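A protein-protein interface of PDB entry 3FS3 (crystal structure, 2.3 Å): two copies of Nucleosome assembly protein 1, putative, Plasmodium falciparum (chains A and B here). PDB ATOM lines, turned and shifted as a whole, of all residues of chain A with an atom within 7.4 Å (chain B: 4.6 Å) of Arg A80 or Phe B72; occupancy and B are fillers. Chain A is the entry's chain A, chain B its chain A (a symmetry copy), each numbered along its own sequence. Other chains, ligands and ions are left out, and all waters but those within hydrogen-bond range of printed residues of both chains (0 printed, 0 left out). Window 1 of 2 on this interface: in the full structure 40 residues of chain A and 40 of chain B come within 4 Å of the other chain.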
ATOM      1  N   TYR A  74       2.354  40.889  27.134  1.00  0.00           N
ATOM      2  CA  TYR A  74       1.098  40.715  27.852  1.00  0.00           C
ATOM      3  C   TYR A  74       0.207  39.705  27.132  1.00  0.00           C
ATOM      4  O   TYR A  74      -0.319  38.781  27.757  1.00  0.00           O
ATOM      5  CB  TYR A  74       0.358  42.048  27.984  1.00  0.00           C
ATOM      6  CG  TYR A  74      -0.878  41.945  28.845  1.00  0.00           C
ATOM      7  CD1 TYR A  74      -0.775  41.725  30.219  1.00  0.00           C
ATOM      8  CD2 TYR A  74      -2.151  42.026  28.285  1.00  0.00           C
ATOM      9  CE1 TYR A  74      -1.909  41.585  31.015  1.00  0.00           C
ATOM     10  CE2 TYR A  74      -3.289  41.889  29.069  1.00  0.00           C
ATOM     11  CZ  TYR A  74      -3.162  41.667  30.433  1.00  0.00           C
ATOM     12  OH  TYR A  74      -4.286  41.516  31.211  1.00  0.00           O
ATOM     13  N   GLU A  75       0.036  39.873  25.821  1.00  0.00           N
ATOM     14  CA  GLU A  75      -0.788  38.933  25.069  1.00  0.00           C
ATOM     15  C   GLU A  75      -0.198  37.517  25.102  1.00  0.00           C
ATOM     16  O   GLU A  75      -0.926  36.538  24.967  1.00  0.00           O
ATOM     17  CB  GLU A  75      -0.975  39.397  23.618  1.00  0.00           C
ATOM     18  CG  GLU A  75      -1.839  40.648  23.476  1.00  0.00           C
ATOM     19  CD  GLU A  75      -2.319  40.876  22.053  1.00  0.00           C
ATOM     20  OE1 GLU A  75      -3.133  40.068  21.558  1.00  0.00           O
ATOM     21  OE2 GLU A  75      -1.882  41.859  21.423  1.00  0.00           O
ATOM     22  N   LEU A  76       1.116  37.410  25.288  1.00  0.00           N
ATOM     23  CA  LEU A  76       1.761  36.098  25.366  1.00  0.00           C
ATOM     24  C   LEU A  76       1.417  35.454  26.714  1.00  0.00           C
ATOM     25  O   LEU A  76       1.182  34.254  26.797  1.00  0.00           O
ATOM     26  CB  LEU A  76       3.281  36.232  25.228  1.00  0.00           C
ATOM     27  CG  LEU A  76       4.100  34.936  25.345  1.00  0.00           C
ATOM     28  CD1 LEU A  76       3.665  33.946  24.274  1.00  0.00           C
ATOM     29  CD2 LEU A  76       5.584  35.247  25.199  1.00  0.00           C
ATOM     30  N   PHE A  77       1.389  36.263  27.767  1.00  0.00           N
ATOM     31  CA  PHE A  77       1.054  35.774  29.100  1.00  0.00           C
ATOM     32  C   PHE A  77      -0.369  35.237  29.070  1.00  0.00           C
ATOM     33  O   PHE A  77      -0.640  34.154  29.579  1.00  0.00           O
ATOM     34  CB  PHE A  77       1.153  36.904  30.129  1.00  0.00           C
ATOM     35  CG  PHE A  77       2.564  37.266  30.516  1.00  0.00           C
ATOM     36  CD1 PHE A  77       3.654  36.783  29.794  1.00  0.00           C
ATOM     37  CD2 PHE A  77       2.802  38.112  31.602  1.00  0.00           C
ATOM     38  CE1 PHE A  77       4.960  37.143  30.142  1.00  0.00           C
ATOM     39  CE2 PHE A  77       4.103  38.478  31.960  1.00  0.00           C
ATOM     40  CZ  PHE A  77       5.185  37.990  31.228  1.00  0.00           C
ATOM     41  N   LEU A  78      -1.273  36.006  28.470  1.00  0.00           N
ATOM     42  CA  LEU A  78      -2.667  35.605  28.354  1.00  0.00           C
ATOM     43  C   LEU A  78      -2.769  34.276  27.630  1.00  0.00           C
ATOM     44  O   LEU A  78      -3.392  33.328  28.114  1.00  0.00           O
ATOM     45  CB  LEU A  78      -3.471  36.648  27.571  1.00  0.00           C
ATOM     46  CG  LEU A  78      -3.946  37.909  28.293  1.00  0.00           C
ATOM     47  CD1 LEU A  78      -4.624  38.844  27.297  1.00  0.00           C
ATOM     48  CD2 LEU A  78      -4.914  37.528  29.405  1.00  0.00           C
ATOM     49  N   LEU A  79      -2.138  34.219  26.465  1.00  0.00           N
ATOM     50  CA  LEU A  79      -2.161  33.033  25.626  1.00  0.00           C
ATOM     51  C   LEU A  79      -1.728  31.782  26.372  1.00  0.00           C
ATOM     52  O   LEU A  79      -2.444  30.787  26.366  1.00  0.00           O
ATOM     53  CB  LEU A  79      -1.280  33.252  24.393  1.00  0.00           C
ATOM     54  CG  LEU A  79      -1.447  32.238  23.264  1.00  0.00           C
ATOM     55  CD1 LEU A  79      -2.896  32.263  22.762  1.00  0.00           C
ATOM     56  CD2 LEU A  79      -0.468  32.565  22.132  1.00  0.00           C
ATOM     57  N   ARG A  80      -0.569  31.828  27.024  1.00  0.00           N
ATOM     58  CA  ARG A  80      -0.083  30.660  27.758  1.00  0.00           C
ATOM     59  C   ARG A  80      -0.999  30.286  28.936  1.00  0.00           C
ATOM     60  O   ARG A  80      -1.156  29.110  29.254  1.00  0.00           O
ATOM     61  CB  ARG A  80       1.354  30.891  28.250  1.00  0.00           C
ATOM     62  CG  ARG A  80       2.404  31.075  27.131  1.00  0.00           C
ATOM     63  CD  ARG A  80       3.818  31.006  27.705  1.00  0.00           C
ATOM     64  NE  ARG A  80       4.883  31.299  26.743  1.00  0.00           N
ATOM     65  CZ  ARG A  80       5.199  30.531  25.703  1.00  0.00           C
ATOM     66  NH1 ARG A  80       4.529  29.408  25.471  1.00  0.00           N
ATOM     67  NH2 ARG A  80       6.201  30.882  24.902  1.00  0.00           N
ATOM     68  N   GLN A  81      -1.613  31.277  29.574  1.00  0.00           N
ATOM     69  CA  GLN A  81      -2.514  31.004  30.689  1.00  0.00           C
ATOM     70  C   GLN A  81      -3.753  30.290  30.173  1.00  0.00           C
ATOM     71  O   GLN A  81      -4.142  29.248  30.694  1.00  0.00           O
ATOM     72  CB  GLN A  81      -2.936  32.299  31.388  1.00  0.00           C
ATOM     73  CG  GLN A  81      -1.800  33.047  32.065  1.00  0.00           C
ATOM     74  CD  GLN A  81      -1.011  32.168  33.011  1.00  0.00           C
ATOM     75  OE1 GLN A  81      -0.379  31.197  32.591  1.00  0.00           O
ATOM     76  NE2 GLN A  81      -1.045  32.500  34.300  1.00  0.00           N
ATOM     77  N   LYS A  82      -4.364  30.857  29.140  1.00  0.00           N
ATOM     78  CA  LYS A  82      -5.556  30.282  28.540  1.00  0.00           C
ATOM     79  C   LYS A  82      -5.386  28.790  28.253  1.00  0.00           C
ATOM     80  O   LYS A  82      -6.186  27.968  28.702  1.00  0.00           O
ATOM     81  CB  LYS A  82      -5.889  31.019  27.243  1.00  0.00           C
ATOM     82  CG  LYS A  82      -6.941  30.338  26.393  1.00  0.00           C
ATOM     83  CD  LYS A  82      -7.056  31.016  25.040  1.00  0.00           C
ATOM     84  CE  LYS A  82      -7.858  30.177  24.058  1.00  0.00           C
ATOM     85  NZ  LYS A  82      -7.930  30.838  22.722  1.00  0.00           N
ATOM     86  N   TYR A  83      -4.347  28.435  27.508  1.00  0.00           N
ATOM     87  CA  TYR A  83      -4.137  27.033  27.185  1.00  0.00           C
ATOM     88  C   TYR A  83      -3.745  26.209  28.399  1.00  0.00           C
ATOM     89  O   TYR A  83      -4.061  25.022  28.473  1.00  0.00           O
ATOM     90  CB  TYR A  83      -3.129  26.902  26.039  1.00  0.00           C
ATOM     91  CG  TYR A  83      -3.784  27.224  24.713  1.00  0.00           C
ATOM     92  CD1 TYR A  83      -4.412  26.228  23.966  1.00  0.00           C
ATOM     93  CD2 TYR A  83      -3.886  28.545  24.268  1.00  0.00           C
ATOM     94  CE1 TYR A  83      -5.135  26.538  22.817  1.00  0.00           C
ATOM     95  CE2 TYR A  83      -4.606  28.866  23.122  1.00  0.00           C
ATOM     96  CZ  TYR A  83      -5.231  27.858  22.402  1.00  0.00           C
ATOM     97  OH  TYR A  83      -5.969  28.172  21.283  1.00  0.00           O
ATOM     98  N   HIS A  84      -3.069  26.828  29.360  1.00  0.00           N
ATOM     99  CA  HIS A  84      -2.722  26.097  30.565  1.00  0.00           C
ATOM    100  C   HIS A  84      -4.029  25.586  31.175  1.00  0.00           C
ATOM    101  O   HIS A  84      -4.105  24.445  31.621  1.00  0.00           O
ATOM    102  CB  HIS A  84      -2.021  26.986  31.585  1.00  0.00           C
ATOM    103  CG  HIS A  84      -1.754  26.294  32.885  1.00  0.00           C
ATOM    104  ND1 HIS A  84      -0.908  25.208  32.988  1.00  0.00           N
ATOM    105  CD2 HIS A  84      -2.250  26.503  34.127  1.00  0.00           C
ATOM    106  CE1 HIS A  84      -0.896  24.781  34.238  1.00  0.00           C
ATOM    107  NE2 HIS A  84      -1.701  25.549  34.949  1.00  0.00           N
ATOM    108  N   ASP A  85      -5.052  26.443  31.176  1.00  0.00           N
ATOM    109  CA  ASP A  85      -6.362  26.090  31.717  1.00  0.00           C
ATOM    110  C   ASP A  85      -7.122  25.114  30.828  1.00  0.00           C
ATOM    111  O   ASP A  85      -7.960  24.353  31.307  1.00  0.00           O
ATOM    112  CB  ASP A  85      -7.211  27.343  31.951  1.00  0.00           C
ATOM    113  CG  ASP A  85      -6.753  28.135  33.166  1.00  0.00           C
ATOM    114  OD1 ASP A  85      -6.634  27.537  34.261  1.00  0.00           O
ATOM    115  OD2 ASP A  85      -6.511  29.354  33.032  1.00  0.00           O
ATOM    116  N   LEU A  86      -6.840  25.136  29.530  1.00  0.00           N
ATOM    117  CA  LEU A  86      -7.491  24.203  28.622  1.00  0.00           C
ATOM    118  C   LEU A  86      -6.863  22.814  28.784  1.00  0.00           C
ATOM    119  O   LEU A  86      -7.542  21.806  28.631  1.00  0.00           O
ATOM    120  CB  LEU A  86      -7.372  24.689  27.170  1.00  0.00           C
ATOM    121  CG  LEU A  86      -8.239  25.921  26.862  1.00  0.00           C
ATOM    122  CD1 LEU A  86      -8.061  26.341  25.422  1.00  0.00           C
ATOM    123  CD2 LEU A  86      -9.706  25.606  27.141  1.00  0.00           C
ATOM    124  N   TYR A  87      -5.573  22.753  29.105  1.00  0.00           N
ATOM    125  CA  TYR A  87      -4.913  21.452  29.290  1.00  0.00           C
ATOM    126  C   TYR A  87      -5.318  20.781  30.605  1.00  0.00           C
ATOM    127  O   TYR A  87      -5.409  19.548  30.687  1.00  0.00           O
ATOM    128  CB  TYR A  87      -3.381  21.589  29.270  1.00  0.00           C
ATOM    129  CG  TYR A  87      -2.791  22.163  27.997  1.00  0.00           C
ATOM    130  CD1 TYR A  87      -3.313  21.836  26.742  1.00  0.00           C
ATOM    131  CD2 TYR A  87      -1.703  23.026  28.048  1.00  0.00           C
ATOM    132  CE1 TYR A  87      -2.759  22.361  25.566  1.00  0.00           C
ATOM    133  CE2 TYR A  87      -1.137  23.556  26.878  1.00  0.00           C
ATOM    134  CZ  TYR A  87      -1.672  23.222  25.645  1.00  0.00           C
ATOM    135  OH  TYR A  87      -1.135  23.763  24.498  1.00  0.00           O
ATOM    136  N   TYR A 147       1.517  26.821  38.499  1.00  0.00           N
ATOM    137  CA  TYR A 147       2.151  28.130  38.616  1.00  0.00           C
ATOM    138  C   TYR A 147       2.107  28.402  40.107  1.00  0.00           C
ATOM    139  O   TYR A 147       1.233  27.886  40.801  1.00  0.00           O
ATOM    140  CB  TYR A 147       1.319  29.226  37.929  1.00  0.00           C
ATOM    141  CG  TYR A 147       1.386  29.255  36.425  1.00  0.00           C
ATOM    142  CD1 TYR A 147       2.575  29.566  35.770  1.00  0.00           C
ATOM    143  CD2 TYR A 147       0.256  28.979  35.654  1.00  0.00           C
ATOM    144  CE1 TYR A 147       2.643  29.602  34.382  1.00  0.00           C
ATOM    145  CE2 TYR A 147       0.311  29.010  34.260  1.00  0.00           C
ATOM    146  CZ  TYR A 147       1.510  29.323  33.631  1.00  0.00           C
ATOM    147  OH  TYR A 147       1.583  29.353  32.256  1.00  0.00           O
ATOM    148  N   GLU A 279       7.706  20.231  30.301  1.00  0.00           N
ATOM    149  CA  GLU A 279       7.336  20.446  28.907  1.00  0.00           C
ATOM    150  C   GLU A 279       7.181  19.204  28.042  1.00  0.00           C
ATOM    151  O   GLU A 279       6.551  19.262  26.990  1.00  0.00           O
ATOM    152  CB  GLU A 279       8.356  21.372  28.249  1.00  0.00           C
ATOM    153  CG  GLU A 279       8.655  22.622  29.046  1.00  0.00           C
ATOM    154  CD  GLU A 279       9.514  23.600  28.277  1.00  0.00           C
ATOM    155  OE1 GLU A 279      10.629  23.215  27.857  1.00  0.00           O
ATOM    156  OE2 GLU A 279       9.071  24.756  28.090  1.00  0.00           O
ATOM    157  N   TYR B  68      -5.649  20.945  21.014  1.00  0.00           N
ATOM    158  CA  TYR B  68      -5.517  22.229  21.685  1.00  0.00           C
ATOM    159  C   TYR B  68      -4.134  22.824  21.445  1.00  0.00           C
ATOM    160  O   TYR B  68      -4.002  24.018  21.189  1.00  0.00           O
ATOM    161  CB  TYR B  68      -5.757  22.080  23.189  1.00  0.00           C
ATOM    162  CG  TYR B  68      -7.213  22.091  23.569  1.00  0.00           C
ATOM    163  CD1 TYR B  68      -8.025  23.176  23.252  1.00  0.00           C
ATOM    164  CD2 TYR B  68      -7.779  21.024  24.248  1.00  0.00           C
ATOM    165  CE1 TYR B  68      -9.371  23.192  23.605  1.00  0.00           C
ATOM    166  CE2 TYR B  68      -9.119  21.031  24.607  1.00  0.00           C
ATOM    167  CZ  TYR B  68      -9.910  22.118  24.284  1.00  0.00           C
ATOM    168  OH  TYR B  68     -11.234  22.130  24.656  1.00  0.00           O
ATOM    169  N   GLU B  69      -3.103  21.991  21.529  1.00  0.00           N
ATOM    170  CA  GLU B  69      -1.749  22.475  21.317  1.00  0.00           C
ATOM    171  C   GLU B  69      -1.572  23.064  19.911  1.00  0.00           C
ATOM    172  O   GLU B  69      -0.873  24.058  19.740  1.00  0.00           O
ATOM    173  CB  GLU B  69      -0.733  21.353  21.547  1.00  0.00           C
ATOM    174  CG  GLU B  69       0.717  21.824  21.453  1.00  0.00           C
ATOM    175  CD  GLU B  69       1.712  20.699  21.652  1.00  0.00           C
ATOM    176  OE1 GLU B  69       1.732  19.766  20.822  1.00  0.00           O
ATOM    177  OE2 GLU B  69       2.468  20.744  22.640  1.00  0.00           O
ATOM    178  N   SER B  70      -2.198  22.451  18.908  1.00  0.00           N
ATOM    179  CA  SER B  70      -2.095  22.958  17.544  1.00  0.00           C
ATOM    180  C   SER B  70      -2.748  24.327  17.472  1.00  0.00           C
ATOM    181  O   SER B  70      -2.263  25.219  16.785  1.00  0.00           O
ATOM    182  CB  SER B  70      -2.789  22.025  16.557  1.00  0.00           C
ATOM    183  OG  SER B  70      -2.151  20.767  16.530  1.00  0.00           O
ATOM    184  N   LYS B  71      -3.855  24.486  18.188  1.00  0.00           N
ATOM    185  CA  LYS B  71      -4.560  25.761  18.200  1.00  0.00           C
ATOM    186  C   LYS B  71      -3.750  26.833  18.935  1.00  0.00           C
ATOM    187  O   LYS B  71      -3.796  28.005  18.563  1.00  0.00           O
ATOM    188  CB  LYS B  71      -5.948  25.585  18.823  1.00  0.00           C
ATOM    189  CG  LYS B  71      -6.845  24.658  18.005  1.00  0.00           C
ATOM    190  CD  LYS B  71      -8.235  24.507  18.609  1.00  0.00           C
ATOM    191  CE  LYS B  71      -9.179  23.728  17.684  1.00  0.00           C
ATOM    192  NZ  LYS B  71      -8.745  22.323  17.413  1.00  0.00           N
ATOM    193  N   PHE B  72      -3.008  26.438  19.969  1.00  0.00           N
ATOM    194  CA  PHE B  72      -2.180  27.398  20.702  1.00  0.00           C
ATOM    195  C   PHE B  72      -1.045  27.815  19.778  1.00  0.00           C
ATOM    196  O   PHE B  72      -0.730  29.001  19.649  1.00  0.00           O
ATOM    197  CB  PHE B  72      -1.574  26.771  21.962  1.00  0.00           C
ATOM    198  CG  PHE B  72      -0.380  27.522  22.500  1.00  0.00           C
ATOM    199  CD1 PHE B  72      -0.546  28.679  23.256  1.00  0.00           C
ATOM    200  CD2 PHE B  72       0.913  27.075  22.236  1.00  0.00           C
ATOM    201  CE1 PHE B  72       0.565  29.384  23.749  1.00  0.00           C
ATOM    202  CE2 PHE B  72       2.029  27.766  22.720  1.00  0.00           C
ATOM    203  CZ  PHE B  72       1.852  28.929  23.483  1.00  0.00           C
ATOM    204  N   GLU B  73      -0.433  26.829  19.134  1.00  0.00           N
ATOM    205  CA  GLU B  73       0.671  27.120  18.232  1.00  0.00           C
ATOM    206  C   GLU B  73       0.211  28.108  17.167  1.00  0.00           C
ATOM    207  O   GLU B  73       0.941  29.024  16.808  1.00  0.00           O
ATOM    208  CB  GLU B  73       1.175  25.842  17.564  1.00  0.00           C
ATOM    209  CG  GLU B  73       2.517  26.014  16.884  1.00  0.00           C
ATOM    210  CD  GLU B  73       2.837  24.897  15.909  1.00  0.00           C
ATOM    211  OE1 GLU B  73       4.032  24.727  15.578  1.00  0.00           O
ATOM    212  OE2 GLU B  73       1.899  24.200  15.462  1.00  0.00           O
ATOM    213  N   TYR B  74      -1.011  27.921  16.671  1.00  0.00           N
ATOM    214  CA  TYR B  74      -1.553  28.808  15.649  1.00  0.00           C
ATOM    215  C   TYR B  74      -1.695  30.226  16.194  1.00  0.00           C
ATOM    216  O   TYR B  74      -1.261  31.187  15.553  1.00  0.00           O
ATOM    217  CB  TYR B  74      -2.914  28.307  15.161  1.00  0.00           C
ATOM    218  CG  TYR B  74      -3.449  29.110  14.000  1.00  0.00           C
ATOM    219  CD1 TYR B  74      -2.838  29.047  12.747  1.00  0.00           C
ATOM    220  CD2 TYR B  74      -4.537  29.964  14.160  1.00  0.00           C
ATOM    221  CE1 TYR B  74      -3.297  29.818  11.682  1.00  0.00           C
ATOM    222  CE2 TYR B  74      -5.004  30.737  13.105  1.00  0.00           C
ATOM    223  CZ  TYR B  74      -4.378  30.661  11.869  1.00  0.00           C
ATOM    224  OH  TYR B  74      -4.828  31.435  10.824  1.00  0.00           O
ATOM    225  N   GLU B  75      -2.299  30.365  17.373  1.00  0.00           N
ATOM    226  CA  GLU B  75      -2.452  31.692  17.960  1.00  0.00           C
ATOM    227  C   GLU B  75      -1.091  32.335  18.258  1.00  0.00           C
ATOM    228  O   GLU B  75      -0.976  33.557  18.289  1.00  0.00           O
ATOM    229  CB  GLU B  75      -3.306  31.640  19.235  1.00  0.00           C
ATOM    230  CG  GLU B  75      -4.775  31.314  18.982  1.00  0.00           C
ATOM    231  CD  GLU B  75      -5.664  31.627  20.173  1.00  0.00           C
ATOM    232  OE1 GLU B  75      -5.825  32.821  20.503  1.00  0.00           O
ATOM    233  OE2 GLU B  75      -6.200  30.683  20.787  1.00  0.00           O
ATOM    234  N   LEU B  76      -0.064  31.515  18.468  1.00  0.00           N
ATOM    235  CA  LEU B  76       1.277  32.040  18.726  1.00  0.00           C
ATOM    236  C   LEU B  76       1.857  32.592  17.418  1.00  0.00           C
ATOM    237  O   LEU B  76       2.521  33.621  17.408  1.00  0.00           O
ATOM    238  CB  LEU B  76       2.193  30.942  19.276  1.00  0.00           C
ATOM    239  CG  LEU B  76       3.655  31.334  19.545  1.00  0.00           C
ATOM    240  CD1 LEU B  76       3.712  32.474  20.552  1.00  0.00           C
ATOM    241  CD2 LEU B  76       4.425  30.131  20.073  1.00  0.00           C
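Among the printed residues, merely in contact across the chains: Tyr A83 with Tyr B68, Arg A80 with Phe B72, Tyr A87 with Glu B69, Tyr A83 with Phe B72, Leu A79 with Phe B72, Leu A79 with Glu B75, Leu A79 with Leu B76, Tyr A87 with Tyr B68, Leu A86 with Tyr B68 and Tyr A87 with Phe B72.
Hydrophobic or aromatic side chains of chain A that line the printed part of chain B: Leu A79, Tyr A83, Leu A86 and Tyr A87. Among the printed residues, 13 pairs touch across the chains.
Of chain B, only Phe B72 comes within 4 Å of Arg A80. Phe B72 touches just these residues of chain A: Leu A79, Arg A80, Tyr A83 and Tyr A87. Of the printed residues of chain A, Tyr B68 touches Tyr A83 (3.2 Å), Leu A86 (3.8 Å) and Tyr A87 (3.8 Å). Of the printed residues of chain B, Leu A79 touches Phe B72 (3.5 Å), Glu B75 (3.6 Å) and Leu B76 (3.8 Å). The nearest printed residue of chain B that does not touch Arg A80 is Leu B76 (5.2 Å). The nearest residue of chain A that does not touch Phe B72 is Leu A76 (5.4 Å).
Positions printed for both chains: 74, 75 and 76.
NZ of Lys A82 is in salt-bridge range of OE2 of Glu B75 (2.6 Å). O of Lys B71 is in hydrogen-bond range of OH of Tyr A83, at 3.5 Å. The side-chain hydroxyl (OH) of Tyr A83 sits at hydrogen-bond distance from the side-chain carboxylate (OE2) of Glu B75, 2.6 Å away.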
